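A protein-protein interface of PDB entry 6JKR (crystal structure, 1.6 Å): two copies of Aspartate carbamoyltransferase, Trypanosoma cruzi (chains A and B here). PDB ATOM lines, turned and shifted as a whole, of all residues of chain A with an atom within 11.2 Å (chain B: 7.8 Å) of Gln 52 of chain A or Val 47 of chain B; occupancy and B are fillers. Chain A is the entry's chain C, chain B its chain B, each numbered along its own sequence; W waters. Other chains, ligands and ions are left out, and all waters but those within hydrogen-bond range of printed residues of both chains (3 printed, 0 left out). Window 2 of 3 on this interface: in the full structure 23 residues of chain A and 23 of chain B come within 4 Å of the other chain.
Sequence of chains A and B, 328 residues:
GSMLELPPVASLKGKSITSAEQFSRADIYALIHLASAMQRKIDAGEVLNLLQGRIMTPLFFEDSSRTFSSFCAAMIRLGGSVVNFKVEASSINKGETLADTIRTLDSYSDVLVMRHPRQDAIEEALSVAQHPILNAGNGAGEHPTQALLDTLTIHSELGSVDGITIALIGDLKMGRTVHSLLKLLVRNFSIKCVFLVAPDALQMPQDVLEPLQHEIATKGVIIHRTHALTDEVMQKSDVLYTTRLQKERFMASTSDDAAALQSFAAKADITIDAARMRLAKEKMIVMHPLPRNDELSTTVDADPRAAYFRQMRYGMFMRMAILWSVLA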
ATOM      1  N   VAL A  47     -40.080  -7.413  11.030  1.00  0.00           N
ATOM      2  CA  VAL A  47     -38.877  -8.095  11.517  1.00  0.00           C
ATOM      3  C   VAL A  47     -37.934  -7.063  12.128  1.00  0.00           C
ATOM      4  O   VAL A  47     -37.561  -6.070  11.478  1.00  0.00           O
ATOM      5  CB  VAL A  47     -38.142  -8.808  10.357  1.00  0.00           C
ATOM      6  CG1 VAL A  47     -36.859  -9.441  10.827  1.00  0.00           C
ATOM      7  CG2 VAL A  47     -39.032  -9.846   9.690  1.00  0.00           C
ATOM      8  N   LEU A  48     -37.540  -7.292  13.377  1.00  0.00           N
ATOM      9  CA  LEU A  48     -36.621  -6.384  14.056  1.00  0.00           C
ATOM     10  C   LEU A  48     -35.194  -6.914  13.986  1.00  0.00           C
ATOM     11  O   LEU A  48     -34.981  -8.143  14.064  1.00  0.00           O
ATOM     12  CB  LEU A  48     -37.095  -6.144  15.495  1.00  0.00           C
ATOM     13  CG  LEU A  48     -38.567  -5.748  15.702  1.00  0.00           C
ATOM     14  CD1 LEU A  48     -38.953  -5.569  17.176  1.00  0.00           C
ATOM     15  CD2 LEU A  48     -38.863  -4.437  14.930  1.00  0.00           C
ATOM     16  N   ASN A  49     -34.213  -6.024  13.803  1.00  0.00           N
ATOM     17  CA  ASN A  49     -32.803  -6.433  13.747  1.00  0.00           C
ATOM     18  C   ASN A  49     -31.912  -5.710  14.765  1.00  0.00           C
ATOM     19  O   ASN A  49     -30.671  -5.642  14.631  1.00  0.00           O
ATOM     20  CB  ASN A  49     -32.236  -6.323  12.318  1.00  0.00           C
ATOM     21  CG  ASN A  49     -31.421  -7.548  11.916  1.00  0.00           C
ATOM     22  OD1 ASN A  49     -31.455  -8.592  12.582  1.00  0.00           O
ATOM     23  ND2 ASN A  49     -30.679  -7.427  10.820  1.00  0.00           N
ATOM     24  N   LEU A  50     -32.542  -5.264  15.837  1.00  0.00           N
ATOM     25  CA  LEU A  50     -31.935  -4.389  16.817  1.00  0.00           C
ATOM     26  C   LEU A  50     -30.684  -4.962  17.478  1.00  0.00           C
ATOM     27  O   LEU A  50     -29.739  -4.229  17.756  1.00  0.00           O
ATOM     28  CB  LEU A  50     -32.973  -4.051  17.875  1.00  0.00           C
ATOM     29  CG  LEU A  50     -34.175  -3.299  17.274  1.00  0.00           C
ATOM     30  CD1 LEU A  50     -35.240  -3.092  18.286  1.00  0.00           C
ATOM     31  CD2 LEU A  50     -33.685  -1.950  16.740  1.00  0.00           C
ATOM     32  N   LEU A  51     -30.690  -6.285  17.708  1.00  0.00           N
ATOM     33  CA  LEU A  51     -29.598  -6.942  18.439  1.00  0.00           C
ATOM     34  C   LEU A  51     -28.849  -7.969  17.603  1.00  0.00           C
ATOM     35  O   LEU A  51     -28.306  -8.916  18.150  1.00  0.00           O
ATOM     36  CB  LEU A  51     -30.117  -7.613  19.742  1.00  0.00           C
ATOM     37  CG  LEU A  51     -30.665  -6.643  20.819  1.00  0.00           C
ATOM     38  CD1 LEU A  51     -31.076  -7.400  22.045  1.00  0.00           C
ATOM     39  CD2 LEU A  51     -29.643  -5.557  21.200  1.00  0.00           C
ATOM     40  N   GLN A  52     -28.776  -7.786  16.282  1.00  0.00           N
ATOM     41  CA  GLN A  52     -28.006  -8.724  15.483  1.00  0.00           C
ATOM     42  C   GLN A  52     -26.567  -8.786  16.014  1.00  0.00           C
ATOM     43  O   GLN A  52     -25.948  -7.731  16.310  1.00  0.00           O
ATOM     44  CB  GLN A  52     -28.014  -8.299  14.003  1.00  0.00           C
ATOM     45  CG  GLN A  52     -27.364  -9.344  13.099  1.00  0.00           C
ATOM     46  CD  GLN A  52     -27.383  -8.937  11.643  1.00  0.00           C
ATOM     47  OE1 GLN A  52     -27.939  -7.890  11.286  1.00  0.00           O
ATOM     48  NE2 GLN A  52     -26.763  -9.758  10.788  1.00  0.00           N
ATOM     49  N   GLY A  53     -26.053 -10.002  16.136  1.00  0.00           N
ATOM     50  CA  GLY A  53     -24.671 -10.211  16.573  1.00  0.00           C
ATOM     51  C   GLY A  53     -24.521 -10.175  18.084  1.00  0.00           C
ATOM     52  O   GLY A  53     -23.400 -10.249  18.586  1.00  0.00           O
ATOM     53  N   ARG A  54     -25.621 -10.063  18.826  1.00  0.00           N
ATOM     54  CA  ARG A  54     -25.553 -10.084  20.292  1.00  0.00           C
ATOM     55  C   ARG A  54     -26.015 -11.446  20.793  1.00  0.00           C
ATOM     56  O   ARG A  54     -26.924 -12.031  20.225  1.00  0.00           O
ATOM     57  CB  ARG A  54     -26.433  -8.997  20.926  1.00  0.00           C
ATOM     58  CG  ARG A  54     -26.197  -7.566  20.402  1.00  0.00           C
ATOM     59  CD  ARG A  54     -24.759  -7.151  20.535  1.00  0.00           C
ATOM     60  NE  ARG A  54     -24.398  -6.847  21.912  1.00  0.00           N
ATOM     61  CZ  ARG A  54     -24.787  -5.768  22.584  1.00  0.00           C
ATOM     62  NH1 ARG A  54     -24.369  -5.599  23.832  1.00  0.00           N
ATOM     63  NH2 ARG A  54     -25.608  -4.878  22.039  1.00  0.00           N
ATOM     64  N   ILE A  55     -25.387 -11.922  21.866  1.00  0.00           N
ATOM     65  CA  ILE A  55     -25.664 -13.267  22.397  1.00  0.00           C
ATOM     66  C   ILE A  55     -26.194 -13.250  23.833  1.00  0.00           C
ATOM     67  O   ILE A  55     -25.650 -12.591  24.720  1.00  0.00           O
ATOM     68  CB  ILE A  55     -24.375 -14.104  22.342  1.00  0.00           C
ATOM     69  CG1 ILE A  55     -23.993 -14.399  20.886  1.00  0.00           C
ATOM     70  CG2 ILE A  55     -24.549 -15.454  23.119  1.00  0.00           C
ATOM     71  CD1 ILE A  55     -22.649 -15.193  20.765  1.00  0.00           C
ATOM     72  N   MET A  56     -27.268 -13.996  24.021  1.00  0.00           N
ATOM     73  CA  MET A  56     -27.776 -14.277  25.353  1.00  0.00           C
ATOM     74  C   MET A  56     -27.467 -15.736  25.676  1.00  0.00           C
ATOM     75  O   MET A  56     -27.665 -16.638  24.837  1.00  0.00           O
ATOM     76  CB  MET A  56     -29.277 -14.026  25.400  1.00  0.00           C
ATOM     77  CG  MET A  56     -29.890 -14.108  26.787  1.00  0.00           C
ATOM     78  SD  MET A  56     -30.574 -15.753  27.065  1.00  0.00           S
ATOM     79  CE  MET A  56     -31.922 -15.750  25.867  1.00  0.00           C
ATOM     80  N   ALA A  74     -37.715 -13.776  22.895  1.00  0.00           N
ATOM     81  CA  ALA A  74     -37.550 -12.308  22.897  1.00  0.00           C
ATOM     82  C   ALA A  74     -36.208 -11.910  22.257  1.00  0.00           C
ATOM     83  O   ALA A  74     -36.151 -10.996  21.392  1.00  0.00           O
ATOM     84  CB  ALA A  74     -37.647 -11.755  24.325  1.00  0.00           C
ATOM     85  N   MET A  75     -35.128 -12.591  22.643  1.00  0.00           N
ATOM     86  CA  MET A  75     -33.799 -12.311  22.056  1.00  0.00           C
ATOM     87  C   MET A  75     -33.832 -12.512  20.533  1.00  0.00           C
ATOM     88  O   MET A  75     -33.395 -11.642  19.769  1.00  0.00           O
ATOM     89  CB  MET A  75     -32.709 -13.171  22.705  1.00  0.00           C
ATOM     90  CG  MET A  75     -31.274 -12.813  22.273  1.00  0.00           C
ATOM     91  SD  MET A  75     -30.880 -11.220  23.032  1.00  0.00           S
ATOM     92  CE  MET A  75     -29.126 -10.998  22.588  1.00  0.00           C
ATOM     93  N   ILE A  76     -34.380 -13.647  20.096  1.00  0.00           N
ATOM     94  CA  ILE A  76     -34.495 -13.954  18.678  1.00  0.00           C
ATOM     95  C   ILE A  76     -35.327 -12.941  17.905  1.00  0.00           C
ATOM     96  O   ILE A  76     -34.969 -12.547  16.767  1.00  0.00           O
ATOM     97  CB  ILE A  76     -35.105 -15.340  18.525  1.00  0.00           C
ATOM     98  CG1 ILE A  76     -34.033 -16.355  18.892  1.00  0.00           C
ATOM     99  CG2 ILE A  76     -35.575 -15.553  17.069  1.00  0.00           C
ATOM    100  CD1 ILE A  76     -34.632 -17.771  19.159  1.00  0.00           C
ATOM    101  N   ARG A  77     -36.423 -12.511  18.517  1.00  0.00           N
ATOM    102  CA  ARG A  77     -37.312 -11.551  17.811  1.00  0.00           C
ATOM    103  C   ARG A  77     -36.751 -10.140  17.762  1.00  0.00           C
ATOM    104  O   ARG A  77     -37.282  -9.280  17.034  1.00  0.00           O
ATOM    105  CB  ARG A  77     -38.718 -11.573  18.406  1.00  0.00           C
ATOM    106  CG  ARG A  77     -39.448 -12.864  18.047  1.00  0.00           C
ATOM    107  CD  ARG A  77     -40.904 -12.805  18.563  1.00  0.00           C
ATOM    108  NE  ARG A  77     -41.600 -14.090  18.360  1.00  0.00           N
ATOM    109  CZ  ARG A  77     -42.086 -14.493  17.184  1.00  0.00           C
ATOM    110  NH1 ARG A  77     -42.004 -13.716  16.107  1.00  0.00           N
ATOM    111  NH2 ARG A  77     -42.686 -15.658  17.085  1.00  0.00           N
ATOM    112  N   LEU A  78     -35.684  -9.893  18.494  1.00  0.00           N
ATOM    113  CA  LEU A  78     -34.957  -8.641  18.345  1.00  0.00           C
ATOM    114  C   LEU A  78     -33.781  -8.799  17.376  1.00  0.00           C
ATOM    115  O   LEU A  78     -32.990  -7.860  17.215  1.00  0.00           O
ATOM    116  CB  LEU A  78     -34.426  -8.200  19.687  1.00  0.00           C
ATOM    117  CG  LEU A  78     -35.437  -7.745  20.733  1.00  0.00           C
ATOM    118  CD1 LEU A  78     -34.755  -7.608  22.113  1.00  0.00           C
ATOM    119  CD2 LEU A  78     -36.097  -6.410  20.281  1.00  0.00           C
ATOM    120  N   GLY A  79     -33.613  -9.978  16.783  1.00  0.00           N
ATOM    121  CA  GLY A  79     -32.490 -10.209  15.870  1.00  0.00           C
ATOM    122  C   GLY A  79     -31.236 -10.786  16.513  1.00  0.00           C
ATOM    123  O   GLY A  79     -30.220 -11.005  15.830  1.00  0.00           O
ATOM    124  N   GLY A  80     -31.305 -11.005  17.828  1.00  0.00           N
ATOM    125  CA  GLY A  80     -30.195 -11.609  18.593  1.00  0.00           C
ATOM    126  C   GLY A  80     -30.122 -13.117  18.514  1.00  0.00           C
ATOM    127  O   GLY A  80     -30.940 -13.765  17.866  1.00  0.00           O
ATOM    128  N   SER A  81     -29.125 -13.665  19.197  1.00  0.00           N
ATOM    129  CA  SER A  81     -28.843 -15.087  19.176  1.00  0.00           C
ATOM    130  C   SER A  81     -28.692 -15.651  20.588  1.00  0.00           C
ATOM    131  O   SER A  81     -28.501 -14.900  21.561  1.00  0.00           O
ATOM    132  CB  SER A  81     -27.551 -15.320  18.412  1.00  0.00           C
ATOM    133  OG  SER A  81     -27.742 -14.913  17.075  1.00  0.00           O
ATOM    134  N   VAL A  82     -28.781 -16.977  20.681  1.00  0.00           N
ATOM    135  CA  VAL A  82     -28.780 -17.662  21.970  1.00  0.00           C
ATOM    136  C   VAL A  82     -27.731 -18.764  21.922  1.00  0.00           C
ATOM    137  O   VAL A  82     -27.656 -19.498  20.932  1.00  0.00           O
ATOM    138  CB  VAL A  82     -30.164 -18.293  22.241  1.00  0.00           C
ATOM    139  CG1 VAL A  82     -30.145 -19.085  23.542  1.00  0.00           C
ATOM    140  CG2 VAL A  82     -31.269 -17.185  22.306  1.00  0.00           C
ATOM    141  N   ASP A 110     -23.254 -11.522  25.636  1.00  0.00           N
ATOM    142  CA  ASP A 110     -23.570 -10.114  25.909  1.00  0.00           C
ATOM    143  C   ASP A 110     -24.443  -9.963  27.135  1.00  0.00           C
ATOM    144  O   ASP A 110     -24.420  -8.905  27.772  1.00  0.00           O
ATOM    145  CB  ASP A 110     -24.223  -9.477  24.678  1.00  0.00           C
ATOM    146  CG  ASP A 110     -23.262  -9.398  23.517  1.00  0.00           C
ATOM    147  OD1 ASP A 110     -22.535  -8.368  23.425  1.00  0.00           O
ATOM    148  OD2 ASP A 110     -23.211 -10.337  22.704  1.00  0.00           O
ATOM    149  N   LEU A 323     -34.624  -6.615  27.123  1.00  0.00           N
ATOM    150  CA  LEU A 323     -33.345  -6.977  26.488  1.00  0.00           C
ATOM    151  C   LEU A 323     -32.843  -5.818  25.621  1.00  0.00           C
ATOM    152  O   LEU A 323     -31.666  -5.499  25.620  1.00  0.00           O
ATOM    153  CB  LEU A 323     -33.498  -8.230  25.645  1.00  0.00           C
ATOM    154  CG  LEU A 323     -33.645  -9.529  26.448  1.00  0.00           C
ATOM    155  CD1 LEU A 323     -34.079 -10.643  25.511  1.00  0.00           C
ATOM    156  CD2 LEU A 323     -32.332  -9.900  27.065  1.00  0.00           C
ATOM    157  N   TRP A 324     -33.753  -5.201  24.906  1.00  0.00           N
ATOM    158  CA  TRP A 324     -33.347  -4.085  24.068  1.00  0.00           C
ATOM    159  C   TRP A 324     -32.843  -2.938  24.925  1.00  0.00           C
ATOM    160  O   TRP A 324     -31.820  -2.323  24.594  1.00  0.00           O
ATOM    161  CB  TRP A 324     -34.502  -3.666  23.170  1.00  0.00           C
ATOM    162  CG  TRP A 324     -34.296  -2.388  22.362  1.00  0.00           C
ATOM    163  CD1 TRP A 324     -35.191  -1.365  22.271  1.00  0.00           C
ATOM    164  CD2 TRP A 324     -33.167  -2.011  21.551  1.00  0.00           C
ATOM    165  NE1 TRP A 324     -34.694  -0.354  21.459  1.00  0.00           N
ATOM    166  CE2 TRP A 324     -33.453  -0.731  21.008  1.00  0.00           C
ATOM    167  CE3 TRP A 324     -31.930  -2.614  21.254  1.00  0.00           C
ATOM    168  CZ2 TRP A 324     -32.556  -0.057  20.164  1.00  0.00           C
ATOM    169  CZ3 TRP A 324     -31.036  -1.945  20.409  1.00  0.00           C
ATOM    170  CH2 TRP A 324     -31.360  -0.677  19.877  1.00  0.00           C
ATOM    171  N   LEU A 327     -29.298  -3.781  26.344  1.00  0.00           N
ATOM    172  CA  LEU A 327     -28.230  -3.982  25.361  1.00  0.00           C
ATOM    173  C   LEU A 327     -28.079  -2.866  24.311  1.00  0.00           C
ATOM    174  O   LEU A 327     -27.140  -2.888  23.512  1.00  0.00           O
ATOM    175  CB  LEU A 327     -28.366  -5.362  24.688  1.00  0.00           C
ATOM    176  CG  LEU A 327     -28.234  -6.576  25.627  1.00  0.00           C
ATOM    177  CD1 LEU A 327     -28.514  -7.867  24.825  1.00  0.00           C
ATOM    178  CD2 LEU A 327     -26.835  -6.595  26.309  1.00  0.00           C
ATOM    179  N   ALA A 328     -29.009  -1.922  24.309  1.00  0.00           N
ATOM    180  CA  ALA A 328     -28.983  -0.772  23.372  1.00  0.00           C
ATOM    181  C   ALA A 328     -27.658  -0.027  23.417  1.00  0.00           C
ATOM    182  O   ALA A 328     -27.178   0.485  22.385  1.00  0.00           O
ATOM    183  CB  ALA A 328     -30.098   0.173  23.685  1.00  0.00           C
ATOM    184  OXT ALA A 328     -27.031   0.053  24.481  1.00  0.00           O
ATOM    185  N   LYS B  41     -12.895  -6.081  15.726  1.00  0.00           N
ATOM    186  CA  LYS B  41     -14.175  -5.778  15.092  1.00  0.00           C
ATOM    187  C   LYS B  41     -15.309  -6.060  16.058  1.00  0.00           C
ATOM    188  O   LYS B  41     -16.175  -5.231  16.267  1.00  0.00           O
ATOM    189  CB  LYS B  41     -14.356  -6.562  13.788  1.00  0.00           C
ATOM    190  CG  LYS B  41     -13.442  -6.082  12.643  1.00  0.00           C
ATOM    191  CD  LYS B  41     -13.810  -6.802  11.347  1.00  0.00           C
ATOM    192  CE  LYS B  41     -12.995  -6.302  10.155  1.00  0.00           C
ATOM    193  NZ  LYS B  41     -13.386  -4.929   9.737  1.00  0.00           N
ATOM    194  N   ILE B  42     -15.281  -7.238  16.679  1.00  0.00           N
ATOM    195  CA  ILE B  42     -16.351  -7.594  17.606  1.00  0.00           C
ATOM    196  C   ILE B  42     -16.429  -6.675  18.826  1.00  0.00           C
ATOM    197  O   ILE B  42     -17.527  -6.268  19.230  1.00  0.00           O
ATOM    198  CB  ILE B  42     -16.228  -9.094  18.064  1.00  0.00           C
ATOM    199  CG1 ILE B  42     -16.412 -10.056  16.873  1.00  0.00           C
ATOM    200  CG2 ILE B  42     -17.161  -9.373  19.245  1.00  0.00           C
ATOM    201  CD1 ILE B  42     -17.758  -9.989  16.083  1.00  0.00           C
ATOM    202  N   ALA B  44     -15.515  -3.661  18.946  1.00  0.00           N
ATOM    203  CA  ALA B  44     -16.006  -2.344  18.459  1.00  0.00           C
ATOM    204  C   ALA B  44     -17.495  -2.372  18.141  1.00  0.00           C
ATOM    205  O   ALA B  44     -18.101  -1.346  17.773  1.00  0.00           O
ATOM    206  CB  ALA B  44     -15.182  -1.879  17.239  1.00  0.00           C
ATOM    207  N   GLY B  45     -18.120  -3.539  18.290  1.00  0.00           N
ATOM    208  CA  GLY B  45     -19.536  -3.671  17.980  1.00  0.00           C
ATOM    209  C   GLY B  45     -19.929  -3.975  16.536  1.00  0.00           C
ATOM    210  O   GLY B  45     -21.127  -3.959  16.197  1.00  0.00           O
ATOM    211  N   GLU B  46     -18.950  -4.259  15.668  1.00  0.00           N
ATOM    212  CA  GLU B  46     -19.261  -4.621  14.277  1.00  0.00           C
ATOM    213  C   GLU B  46     -19.973  -5.963  14.212  1.00  0.00           C
ATOM    214  O   GLU B  46     -19.634  -6.901  14.956  1.00  0.00           O
ATOM    215  CB  GLU B  46     -18.020  -4.630  13.356  1.00  0.00           C
ATOM    216  CG  GLU B  46     -18.351  -4.934  11.867  1.00  0.00           C
ATOM    217  CD  GLU B  46     -17.146  -4.872  10.933  1.00  0.00           C
ATOM    218  OE1 GLU B  46     -17.270  -5.285   9.760  1.00  0.00           O
ATOM    219  OE2 GLU B  46     -16.082  -4.425  11.374  1.00  0.00           O
ATOM    220  N   VAL B  47     -20.948  -6.039  13.319  1.00  0.00           N
ATOM    221  CA  VAL B  47     -21.698  -7.264  13.075  1.00  0.00           C
ATOM    222  C   VAL B  47     -21.129  -7.961  11.847  1.00  0.00           C
ATOM    223  O   VAL B  47     -21.055  -7.374  10.756  1.00  0.00           O
ATOM    224  CB  VAL B  47     -23.192  -6.981  12.900  1.00  0.00           C
ATOM    225  CG1 VAL B  47     -23.938  -8.291  12.620  1.00  0.00           C
ATOM    226  CG2 VAL B  47     -23.742  -6.342  14.169  1.00  0.00           C
ATOM    227  N   LEU B  48     -20.687  -9.199  12.011  1.00  0.00           N
ATOM    228  CA  LEU B  48     -20.115  -9.933  10.876  1.00  0.00           C
ATOM    229  C   LEU B  48     -21.161 -10.847  10.261  1.00  0.00           C
ATOM    230  O   LEU B  48     -21.922 -11.475  10.985  1.00  0.00           O
ATOM    231  CB  LEU B  48     -18.885 -10.712  11.311  1.00  0.00           C
ATOM    232  CG  LEU B  48     -17.803  -9.994  12.110  1.00  0.00           C
ATOM    233  CD1 LEU B  48     -16.621 -10.924  12.388  1.00  0.00           C
ATOM    234  CD2 LEU B  48     -17.287  -8.725  11.384  1.00  0.00           C
ATOM    235  N   ASN B  49     -21.207 -10.930   8.938  1.00  0.00           N
ATOM    236  CA  ASN B  49     -22.166 -11.791   8.252  1.00  0.00           C
ATOM    237  C   ASN B  49     -21.551 -12.874   7.366  1.00  0.00           C
ATOM    238  O   ASN B  49     -22.229 -13.456   6.476  1.00  0.00           O
ATOM    239  CB  ASN B  49     -23.191 -10.963   7.471  1.00  0.00           C
ATOM    240  CG  ASN B  49     -24.373 -10.591   8.307  1.00  0.00           C
ATOM    241  OD1 ASN B  49     -24.681  -9.404   8.473  1.00  0.00           O
ATOM    242  ND2 ASN B  49     -25.062 -11.601   8.848  1.00  0.00           N
ATOM    243  N   LEU B  50     -20.293 -13.191   7.655  1.00  0.00           N
ATOM    244  CA  LEU B  50     -19.458 -14.003   6.792  1.00  0.00           C
ATOM    245  C   LEU B  50     -20.013 -15.388   6.522  1.00  0.00           C
ATOM    246  O   LEU B  50     -19.823 -15.923   5.421  1.00  0.00           O
ATOM    247  CB  LEU B  50     -18.043 -14.133   7.366  1.00  0.00           C
ATOM    248  CG  LEU B  50     -17.312 -12.781   7.504  1.00  0.00           C
ATOM    249  CD1 LEU B  50     -16.038 -12.916   8.311  1.00  0.00           C
ATOM    250  CD2 LEU B  50     -17.017 -12.195   6.139  1.00  0.00           C
ATOM    251  N   GLN B  52     -23.382 -16.423   7.006  1.00  0.00           N
ATOM    252  CA  GLN B  52     -24.831 -16.540   6.928  1.00  0.00           C
ATOM    253  C   GLN B  52     -25.261 -17.777   6.125  1.00  0.00           C
ATOM    254  O   GLN B  52     -24.689 -18.071   5.065  1.00  0.00           O
ATOM    255  CB  GLN B  52     -25.464 -15.268   6.326  1.00  0.00           C
ATOM    256  CG  GLN B  52     -26.985 -15.236   6.532  1.00  0.00           C
ATOM    257  CD  GLN B  52     -27.685 -14.034   5.879  1.00  0.00           C
ATOM    258  OE1 GLN B  52     -27.051 -13.195   5.239  1.00  0.00           O
ATOM    259  NE2 GLN B  52     -29.014 -13.964   6.042  1.00  0.00           N
ATOM    260  N   ILE B  76     -21.900 -18.098  15.703  1.00  0.00           N
ATOM    261  CA  ILE B  76     -22.957 -17.088  15.747  1.00  0.00           C
ATOM    262  C   ILE B  76     -22.359 -15.710  15.418  1.00  0.00           C
ATOM    263  O   ILE B  76     -22.976 -14.930  14.651  1.00  0.00           O
ATOM    264  CB  ILE B  76     -23.638 -17.061  17.112  1.00  0.00           C
ATOM    265  CG1 ILE B  76     -24.547 -18.282  17.240  1.00  0.00           C
ATOM    266  CG2 ILE B  76     -24.432 -15.738  17.268  1.00  0.00           C
ATOM    267  CD1 ILE B  76     -24.942 -18.603  18.702  1.00  0.00           C
ATOM    268  N   ARG B  77     -21.176 -15.436  15.954  1.00  0.00           N
ATOM    269  CA  ARG B  77     -20.573 -14.100  15.747  1.00  0.00           C
ATOM    270  C   ARG B  77     -20.017 -13.960  14.350  1.00  0.00           C
ATOM    271  O   ARG B  77     -19.708 -12.837  13.938  1.00  0.00           O
ATOM    272  CB  ARG B  77     -19.526 -13.775  16.814  1.00  0.00           C
ATOM    273  CG  ARG B  77     -20.133 -13.568  18.202  1.00  0.00           C
ATOM    274  CD  ARG B  77     -19.083 -13.150  19.207  1.00  0.00           C
ATOM    275  NE  ARG B  77     -19.680 -13.044  20.549  1.00  0.00           N
ATOM    276  CZ  ARG B  77     -20.419 -12.018  20.957  1.00  0.00           C
ATOM    277  NH1 ARG B  77     -20.647 -10.983  20.142  1.00  0.00           N
ATOM    278  NH2 ARG B  77     -20.903 -12.012  22.203  1.00  0.00           N
ATOM    279  N   LEU B  78     -19.890 -15.062  13.617  1.00  0.00           N
ATOM    280  CA  LEU B  78     -19.579 -14.971  12.168  1.00  0.00           C
ATOM    281  C   LEU B  78     -20.843 -14.869  11.295  1.00  0.00           C
ATOM    282  O   LEU B  78     -20.749 -14.821  10.075  1.00  0.00           O
ATOM    283  CB  LEU B  78     -18.701 -16.139  11.740  1.00  0.00           C
ATOM    284  CG  LEU B  78     -17.283 -16.227  12.297  1.00  0.00           C
ATOM    285  CD1 LEU B  78     -16.739 -17.618  12.116  1.00  0.00           C
ATOM    286  CD2 LEU B  78     -16.373 -15.230  11.598  1.00  0.00           C
ATOM    287  N   GLY B  79     -22.019 -14.876  11.916  1.00  0.00           N
ATOM    288  CA  GLY B  79     -23.264 -14.862  11.163  1.00  0.00           C
ATOM    289  C   GLY B  79     -23.832 -16.230  10.841  1.00  0.00           C
ATOM    290  O   GLY B  79     -24.886 -16.317  10.218  1.00  0.00           O
HETATM  291  O   HOH W   1     -21.042 -10.091  17.338  1.00  0.00           O
HETATM  292  O   HOH W   2     -21.099  -8.275  21.215  1.00  0.00           O
HETATM  293  O   HOH W   3     -24.848 -11.726  11.579  1.00  0.00           O
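Hydrophobic or aromatic side chains of chain A that line the printed part of chain B: Ile 55.
Along chain A the printed residues that touch a printed residue of chain B span positions 52 to 110.
Hydrophobic or aromatic side chains of chain B that line the printed part of chain A: Val 47 and Ile 76.
Among the printed residues, 8 pairs touch across the chains.
N of Asp 110 of chain A lies within hydrogen-bond range of O of Ile 55 of chain A (2.8 Å).
ND2 of Asn 49 of chain A is in hydrogen-bond range of OE1 of Gln 52 of chain A (2.8 Å).
The backbone carbonyl oxygen (O) of Arg 54 of chain A sits at hydrogen-bond distance from the backbone NH (N) of Ser 81 of chain A (2.9 Å).
The backbone NH (N) of Met 56 of chain A lies within hydrogen-bond range of the backbone carbonyl oxygen (O) of Ser 81 of chain A, 2.9 Å away.
The guanidinium group of Arg 54 of chain A is in salt-bridge range of the side-chain carboxylate of Asp 110 of chain A (2.8 Å).
Among the printed residues, pairs that only touch across the chains: Ser 81 of chain A with Ile 76 of chain B, Gln 52 of chain A with Val 47 of chain B, Val 82 of chain A with Ile 76 of chain B, Ile 55 of chain A with Arg 77 of chain B and Ile 55 of chain A with Ile 76 of chain B.
Water W2 bridges the side-chain carboxylate of Asp 110 of chain A (2.6 Å) and the guanidinium group of Arg 77 of chain B (2.9 Å).
Water W1 lies within hydrogen-bond range of O of Gly 53 of chain A and NH1 of Arg 77 of chain B.
Water W3 lies within hydrogen-bond range of ND2 of Asn 49 of chain B (2.7 Å), NE2 of Gln 52 of chain A (2.9 Å) and O of Leu 48 of chain B (3.0 Å).
Gln 52 of chain A touches Val 47 of chain B, but with the chains exchanged Val 47 of chain A does not touch Gln 52 of chain B (10.2 Å).
Gln 52 of chain A touches Asn 49 of chain B, but with the chains exchanged Asn 49 of chain A does not touch Gln 52 of chain B (8.3 Å).
Positions printed for both chains: 47, 48, 49, 50, 52, 76, 77, 78 and 79.
The side-chain amide nitrogen (NE2) of Gln 52 of chain A sits at hydrogen-bond distance from the side-chain amide oxygen (OD1) of Asn 49 of chain B, 3.1 Å away.
The side-chain carboxylate (OD2) of Asp 110 of chain A is in salt-bridge range of the guanidinium group (NH2) of Arg 77 of chain B, at 2.9 Å.
The backbone carbonyl oxygen (O) of Gly 53 of chain A is in hydrogen-bond range of the guanidinium group (NH1) of Arg 77 of chain B.
Of the printed residues of chain B, Gln 52 of chain A touches Val 47 and Asn 49.
No residue of chain A comes within 4 Å of Leu 48 of chain B.
No residue of chain A comes within 4 Å of Gly 79 of chain B.
Of the printed residues of chain B, Ile 55 of chain A touches Ile 76 and Arg 77.
Of the printed residues of chain B, Val 82 of chain A touches Ile 76 (3.6 Å).
Of the printed residues of chain B, Gly 53 of chain A touches Arg 77.
Of the printed residues of chain B, Asp 110 of chain A touches Arg 77.
Of the printed residues of chain B, Ser 81 of chain A touches Ile 76 (3.3 Å).
Ala 74 of chain A touches none of the printed residues of chain B.
Ala 44 of chain B touches none of the printed residues of chain A.
The nearest printed residue of chain B that does not touch Asp 110 of chain A is Ile 42 of chain B (6.9 Å).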
